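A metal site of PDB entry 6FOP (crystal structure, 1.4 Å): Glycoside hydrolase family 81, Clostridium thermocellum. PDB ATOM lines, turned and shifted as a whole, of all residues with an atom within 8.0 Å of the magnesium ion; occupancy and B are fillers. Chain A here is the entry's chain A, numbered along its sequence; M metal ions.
The side-chain amide nitrogen of Asn 47 sits close to the backbone NH of Ser 50, 3.3 Å away. The backbone NH (N) of Ala 102 sits at hydrogen-bond distance from the backbone carbonyl oxygen (O) of Gln 48 (2.9 Å). N of Tyr 49 sits close to ND2 of Asn 47, at 3.1 Å. The backbone NH of Ala 104 lies within hydrogen-bond range of the backbone carbonyl oxygen of Tyr 26, at 2.9 Å. O of Pro 100 is in hydrogen-bond range of NE2 of Gln 48 (2.8 Å). The side-chain hydroxyl (OH) of Tyr 49 sits at hydrogen-bond distance from the backbone carbonyl oxygen (O) of Pro 100 (3.4 Å). The backbone NH (N) of Tyr 26 sits at hydrogen-bond distance from the backbone carbonyl oxygen (O) of Leu 45 (2.9 Å).
Residues that only touch the magnesium ion: Tyr 26 (3.5 Å). Six residues have an atom within 4 Å of the magnesium ion: Tyr 26, Ile 44, Asn 47, Gln 48, Tyr 49 and Ala 102. Along chain A the residues within 4 Å of the magnesium ion span positions 26 to 102. The nearest printed residue that does not touch the magnesium ion is Ser 43 (4.4 Å).
The magnesium ion is bound by O of Ala 102 (2.2 Å), O of Asn 47 (2.3 Å), O of Ile 44 (2.3 Å) and O of Tyr 49 (2.4 Å). The magnesium ion has four donor atoms within binding distance. Slightly farther from the magnesium ion lies O of Gln 48 (2.7 Å).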
ATOM      1  N   ILE A  25     -15.500  17.569 -26.752  1.00  0.00           N
ATOM      2  CA  ILE A  25     -14.262  17.433 -27.515  1.00  0.00           C
ATOM      3  C   ILE A  25     -13.675  18.821 -27.724  1.00  0.00           C
ATOM      4  O   ILE A  25     -14.293  19.678 -28.368  1.00  0.00           O
ATOM      5  CB  ILE A  25     -14.461  16.725 -28.861  1.00  0.00           C
ATOM      6  CG1 ILE A  25     -15.163  15.376 -28.666  1.00  0.00           C
ATOM      7  CG2 ILE A  25     -13.094  16.476 -29.524  1.00  0.00           C
ATOM      8  CD1 ILE A  25     -15.375  14.570 -29.927  1.00  0.00           C
ATOM      9  N   TYR A  26     -12.489  19.047 -27.172  1.00  0.00           N
ATOM     10  CA  TYR A  26     -11.827  20.345 -27.220  1.00  0.00           C
ATOM     11  C   TYR A  26     -11.097  20.462 -28.568  1.00  0.00           C
ATOM     12  O   TYR A  26      -9.876  20.299 -28.699  1.00  0.00           O
ATOM     13  CB  TYR A  26     -10.921  20.570 -25.982  1.00  0.00           C
ATOM     14  CG  TYR A  26     -11.716  20.790 -24.738  1.00  0.00           C
ATOM     15  CD1 TYR A  26     -12.189  22.068 -24.411  1.00  0.00           C
ATOM     16  CD2 TYR A  26     -12.031  19.725 -23.864  1.00  0.00           C
ATOM     17  CE1 TYR A  26     -12.957  22.275 -23.271  1.00  0.00           C
ATOM     18  CE2 TYR A  26     -12.786  19.929 -22.722  1.00  0.00           C
ATOM     19  CZ  TYR A  26     -13.239  21.207 -22.419  1.00  0.00           C
ATOM     20  OH  TYR A  26     -13.980  21.432 -21.294  1.00  0.00           O
ATOM     21  N   LYS A  27     -11.909  20.747 -29.580  1.00  0.00           N
ATOM     22  CA  LYS A  27     -11.476  20.943 -30.952  1.00  0.00           C
ATOM     23  C   LYS A  27     -12.124  22.229 -31.475  1.00  0.00           C
ATOM     24  O   LYS A  27     -13.163  22.677 -30.957  1.00  0.00           O
ATOM     25  CB  LYS A  27     -11.831  19.742 -31.853  1.00  0.00           C
ATOM     26  CG  LYS A  27     -13.316  19.444 -31.975  1.00  0.00           C
ATOM     27  CD  LYS A  27     -13.550  18.282 -32.934  1.00  0.00           C
ATOM     28  CE  LYS A  27     -14.941  17.705 -32.788  1.00  0.00           C
ATOM     29  NZ  LYS A  27     -15.973  18.648 -33.269  1.00  0.00           N
ATOM     30  N   GLU A  41      -0.498  13.753 -28.670  1.00  0.00           N
ATOM     31  CA  GLU A  41      -1.172  15.049 -28.595  1.00  0.00           C
ATOM     32  C   GLU A  41      -2.587  14.946 -27.998  1.00  0.00           C
ATOM     33  O   GLU A  41      -3.271  15.945 -27.810  1.00  0.00           O
ATOM     34  CB  GLU A  41      -1.228  15.715 -29.965  1.00  0.00           C
ATOM     35  CG  GLU A  41      -2.308  15.171 -30.917  1.00  0.00           C
ATOM     36  CD  GLU A  41      -2.069  13.804 -31.498  1.00  0.00           C
ATOM     37  OE1 GLU A  41      -0.921  13.333 -31.501  1.00  0.00           O
ATOM     38  OE2 GLU A  41      -3.063  13.244 -32.063  1.00  0.00           O
ATOM     39  N   SER A  42      -3.051  13.724 -27.713  1.00  0.00           N
ATOM     40  CA  SER A  42      -4.467  13.478 -27.482  1.00  0.00           C
ATOM     41  C   SER A  42      -5.088  14.210 -26.328  1.00  0.00           C
ATOM     42  O   SER A  42      -6.281  14.499 -26.371  1.00  0.00           O
ATOM     43  CB  SER A  42      -4.717  11.977 -27.367  1.00  0.00           C
ATOM     44  OG  SER A  42      -4.339  11.326 -28.553  1.00  0.00           O
ATOM     45  N   SER A  43      -4.311  14.485 -25.274  1.00  0.00           N
ATOM     46  CA  SER A  43      -4.927  15.121 -24.083  1.00  0.00           C
ATOM     47  C   SER A  43      -5.470  16.534 -24.334  1.00  0.00           C
ATOM     48  O   SER A  43      -6.360  16.987 -23.609  1.00  0.00           O
ATOM     49  CB  SER A  43      -3.954  15.158 -22.903  1.00  0.00           C
ATOM     50  OG  SER A  43      -2.945  16.153 -23.079  1.00  0.00           O
ATOM     51  N   ILE A  44      -4.995  17.176 -25.387  1.00  0.00           N
ATOM     52  CA  ILE A  44      -5.582  18.444 -25.833  1.00  0.00           C
ATOM     53  C   ILE A  44      -7.071  18.334 -26.094  1.00  0.00           C
ATOM     54  O   ILE A  44      -7.828  19.245 -25.733  1.00  0.00           O
ATOM     55  CB  ILE A  44      -4.878  19.001 -27.074  1.00  0.00           C
ATOM     56  CG1 ILE A  44      -3.387  19.234 -26.825  1.00  0.00           C
ATOM     57  CG2 ILE A  44      -5.523  20.290 -27.538  1.00  0.00           C
ATOM     58  CD1 ILE A  44      -2.581  19.431 -28.085  1.00  0.00           C
ATOM     59  N   LEU A  45      -7.491  17.211 -26.684  1.00  0.00           N
ATOM     60  CA  LEU A  45      -8.884  16.977 -27.057  1.00  0.00           C
ATOM     61  C   LEU A  45      -9.777  16.649 -25.876  1.00  0.00           C
ATOM     62  O   LEU A  45     -10.967  16.995 -25.885  1.00  0.00           O
ATOM     63  CB  LEU A  45      -8.978  15.831 -28.079  1.00  0.00           C
ATOM     64  CG  LEU A  45      -8.384  16.145 -29.456  1.00  0.00           C
ATOM     65  CD1 LEU A  45      -7.976  14.856 -30.154  1.00  0.00           C
ATOM     66  CD2 LEU A  45      -9.341  16.963 -30.300  1.00  0.00           C
ATOM     67  N   TRP A  46      -9.229  15.927 -24.882  1.00  0.00           N
ATOM     68  CA  TRP A  46     -10.044  15.394 -23.794  1.00  0.00           C
ATOM     69  C   TRP A  46     -10.124  16.321 -22.573  1.00  0.00           C
ATOM     70  O   TRP A  46     -11.105  16.287 -21.817  1.00  0.00           O
ATOM     71  CB  TRP A  46      -9.472  14.028 -23.359  1.00  0.00           C
ATOM     72  CG  TRP A  46      -9.579  12.903 -24.367  1.00  0.00           C
ATOM     73  CD1 TRP A  46      -8.772  12.694 -25.448  1.00  0.00           C
ATOM     74  CD2 TRP A  46     -10.478  11.804 -24.320  1.00  0.00           C
ATOM     75  NE1 TRP A  46      -9.128  11.527 -26.100  1.00  0.00           N
ATOM     76  CE2 TRP A  46     -10.188  10.963 -25.417  1.00  0.00           C
ATOM     77  CE3 TRP A  46     -11.505  11.438 -23.447  1.00  0.00           C
ATOM     78  CZ2 TRP A  46     -10.869   9.770 -25.649  1.00  0.00           C
ATOM     79  CZ3 TRP A  46     -12.194  10.268 -23.694  1.00  0.00           C
ATOM     80  CH2 TRP A  46     -11.867   9.451 -24.773  1.00  0.00           C
ATOM     81  N   ASN A  47      -9.061  17.090 -22.348  1.00  0.00           N
ATOM     82  CA  ASN A  47      -8.939  17.963 -21.195  1.00  0.00           C
ATOM     83  C   ASN A  47      -9.212  19.415 -21.624  1.00  0.00           C
ATOM     84  O   ASN A  47      -8.966  19.786 -22.754  1.00  0.00           O
ATOM     85  CB  ASN A  47      -7.514  17.756 -20.646  1.00  0.00           C
ATOM     86  CG  ASN A  47      -7.301  18.349 -19.284  1.00  0.00           C
ATOM     87  OD1 ASN A  47      -7.607  17.752 -18.235  1.00  0.00           O
ATOM     88  ND2 ASN A  47      -6.730  19.513 -19.289  1.00  0.00           N
ATOM     89  N   GLN A  48      -9.730  20.227 -20.689  1.00  0.00           N
ATOM     90  CA  GLN A  48      -9.937  21.652 -20.960  1.00  0.00           C
ATOM     91  C   GLN A  48      -8.669  22.259 -21.588  1.00  0.00           C
ATOM     92  O   GLN A  48      -8.722  22.938 -22.608  1.00  0.00           O
ATOM     93  CB  GLN A  48     -10.303  22.348 -19.652  1.00  0.00           C
ATOM     94  CG  GLN A  48     -10.512  23.836 -19.752  1.00  0.00           C
ATOM     95  CD  GLN A  48     -10.937  24.459 -18.433  1.00  0.00           C
ATOM     96  OE1 GLN A  48     -11.000  23.797 -17.408  1.00  0.00           O
ATOM     97  NE2 GLN A  48     -11.198  25.743 -18.458  1.00  0.00           N
ATOM     98  N   TYR A  49      -7.541  22.053 -20.907  1.00  0.00           N
ATOM     99  CA  TYR A  49      -6.258  22.508 -21.383  1.00  0.00           C
ATOM    100  C   TYR A  49      -5.526  21.306 -22.018  1.00  0.00           C
ATOM    101  O   TYR A  49      -5.901  20.902 -23.103  1.00  0.00           O
ATOM    102  CB  TYR A  49      -5.507  23.236 -20.242  1.00  0.00           C
ATOM    103  CG  TYR A  49      -6.224  24.499 -19.810  1.00  0.00           C
ATOM    104  CD1 TYR A  49      -6.269  25.613 -20.635  1.00  0.00           C
ATOM    105  CD2 TYR A  49      -6.930  24.547 -18.611  1.00  0.00           C
ATOM    106  CE1 TYR A  49      -6.959  26.756 -20.257  1.00  0.00           C
ATOM    107  CE2 TYR A  49      -7.588  25.684 -18.218  1.00  0.00           C
ATOM    108  CZ  TYR A  49      -7.623  26.776 -19.043  1.00  0.00           C
ATOM    109  OH  TYR A  49      -8.328  27.889 -18.649  1.00  0.00           O
ATOM    110  N   SER A  50      -4.525  20.743 -21.342  1.00  0.00           N
ATOM    111  CA  SER A  50      -3.943  19.485 -21.723  1.00  0.00           C
ATOM    112  C   SER A  50      -3.227  18.909 -20.529  1.00  0.00           C
ATOM    113  O   SER A  50      -3.046  19.593 -19.502  1.00  0.00           O
ATOM    114  CB  SER A  50      -2.920  19.636 -22.867  1.00  0.00           C
ATOM    115  OG  SER A  50      -1.654  20.137 -22.429  1.00  0.00           O
ATOM    116  N   LEU A  51      -2.767  17.675 -20.682  1.00  0.00           N
ATOM    117  CA  LEU A  51      -1.725  17.097 -19.830  1.00  0.00           C
ATOM    118  C   LEU A  51      -0.399  17.311 -20.577  1.00  0.00           C
ATOM    119  O   LEU A  51      -0.387  17.878 -21.685  1.00  0.00           O
ATOM    120  CB  LEU A  51      -1.986  15.600 -19.551  1.00  0.00           C
ATOM    121  CG  LEU A  51      -2.935  15.313 -18.386  1.00  0.00           C
ATOM    122  CD1 LEU A  51      -2.310  15.682 -17.046  1.00  0.00           C
ATOM    123  CD2 LEU A  51      -4.304  15.936 -18.536  1.00  0.00           C
ATOM    124  N   PHE A  62      -0.461  22.804 -21.967  1.00  0.00           N
ATOM    125  CA  PHE A  62      -1.391  23.950 -22.025  1.00  0.00           C
ATOM    126  C   PHE A  62      -1.956  24.190 -20.635  1.00  0.00           C
ATOM    127  O   PHE A  62      -2.180  23.256 -19.877  1.00  0.00           O
ATOM    128  CB  PHE A  62      -2.521  23.673 -23.033  1.00  0.00           C
ATOM    129  CG  PHE A  62      -2.038  23.633 -24.462  1.00  0.00           C
ATOM    130  CD1 PHE A  62      -1.532  22.455 -25.007  1.00  0.00           C
ATOM    131  CD2 PHE A  62      -2.090  24.777 -25.265  1.00  0.00           C
ATOM    132  CE1 PHE A  62      -1.067  22.424 -26.301  1.00  0.00           C
ATOM    133  CE2 PHE A  62      -1.616  24.745 -26.565  1.00  0.00           C
ATOM    134  CZ  PHE A  62      -1.118  23.555 -27.083  1.00  0.00           C
ATOM    135  N   PRO A 100      -9.653  30.400 -21.898  1.00  0.00           N
ATOM    136  CA  PRO A 100     -10.666  29.497 -21.338  1.00  0.00           C
ATOM    137  C   PRO A 100     -10.393  28.016 -21.579  1.00  0.00           C
ATOM    138  O   PRO A 100     -10.885  27.185 -20.821  1.00  0.00           O
ATOM    139  CB  PRO A 100     -11.942  29.906 -22.087  1.00  0.00           C
ATOM    140  CG  PRO A 100     -11.474  30.462 -23.358  1.00  0.00           C
ATOM    141  CD  PRO A 100     -10.170  31.154 -23.049  1.00  0.00           C
ATOM    142  N   ASP A 101      -9.593  27.688 -22.583  1.00  0.00           N
ATOM    143  CA  ASP A 101      -9.296  26.288 -22.944  1.00  0.00           C
ATOM    144  C   ASP A 101      -8.200  26.255 -23.991  1.00  0.00           C
ATOM    145  O   ASP A 101      -7.758  27.316 -24.453  1.00  0.00           O
ATOM    146  CB  ASP A 101     -10.550  25.545 -23.426  1.00  0.00           C
ATOM    147  CG  ASP A 101     -11.224  26.177 -24.636  1.00  0.00           C
ATOM    148  OD1 ASP A 101     -10.557  26.625 -25.574  1.00  0.00           O
ATOM    149  OD2 ASP A 101     -12.477  26.160 -24.679  1.00  0.00           O
ATOM    150  N   ALA A 102      -7.769  25.050 -24.373  1.00  0.00           N
ATOM    151  CA  ALA A 102      -6.918  24.833 -25.532  1.00  0.00           C
ATOM    152  C   ALA A 102      -7.618  23.780 -26.374  1.00  0.00           C
ATOM    153  O   ALA A 102      -8.002  22.713 -25.842  1.00  0.00           O
ATOM    154  CB  ALA A 102      -5.546  24.364 -25.122  1.00  0.00           C
ATOM    155  N   ARG A 103      -7.732  24.072 -27.676  1.00  0.00           N
ATOM    156  CA  ARG A 103      -8.466  23.218 -28.612  1.00  0.00           C
ATOM    157  C   ARG A 103      -7.607  22.808 -29.791  1.00  0.00           C
ATOM    158  O   ARG A 103      -6.876  23.612 -30.347  1.00  0.00           O
ATOM    159  CB  ARG A 103      -9.700  23.922 -29.133  1.00  0.00           C
ATOM    160  CG  ARG A 103     -10.745  24.157 -28.052  1.00  0.00           C
ATOM    161  CD  ARG A 103     -11.910  25.005 -28.504  1.00  0.00           C
ATOM    162  NE  ARG A 103     -12.918  25.063 -27.435  1.00  0.00           N
ATOM    163  CZ  ARG A 103     -14.008  24.285 -27.354  1.00  0.00           C
ATOM    164  NH1 ARG A 103     -14.304  23.362 -28.273  1.00  0.00           N
ATOM    165  NH2 ARG A 103     -14.820  24.428 -26.309  1.00  0.00           N
ATOM    166  N   ALA A 104      -7.722  21.539 -30.210  1.00  0.00           N
ATOM    167  CA  ALA A 104      -6.999  21.091 -31.407  1.00  0.00           C
ATOM    168  C   ALA A 104      -7.694  21.639 -32.656  1.00  0.00           C
ATOM    169  O   ALA A 104      -8.894  21.513 -32.805  1.00  0.00           O
ATOM    170  CB  ALA A 104      -6.929  19.571 -31.477  1.00  0.00           C
ATOM    171  N   ALA A 114      -2.813  23.778 -32.161  1.00  0.00           N
ATOM    172  CA  ALA A 114      -3.829  24.035 -31.130  1.00  0.00           C
ATOM    173  C   ALA A 114      -4.035  25.533 -30.953  1.00  0.00           C
ATOM    174  O   ALA A 114      -3.094  26.303 -31.131  1.00  0.00           O
ATOM    175  CB  ALA A 114      -3.413  23.409 -29.802  1.00  0.00           C
ATOM    176  N   VAL A 115      -5.253  25.903 -30.588  1.00  0.00           N
ATOM    177  CA  VAL A 115      -5.622  27.307 -30.446  1.00  0.00           C
ATOM    178  C   VAL A 115      -6.124  27.556 -29.035  1.00  0.00           C
ATOM    179  O   VAL A 115      -6.922  26.774 -28.492  1.00  0.00           O
ATOM    180  CB  VAL A 115      -6.751  27.681 -31.441  1.00  0.00           C
ATOM    181  CG1 VAL A 115      -7.266  29.104 -31.178  1.00  0.00           C
ATOM    182  CG2 VAL A 115      -6.268  27.558 -32.862  1.00  0.00           C
HETATM  183 MG    MG M   1      -7.928  21.070 -24.325  1.00  0.00          MG
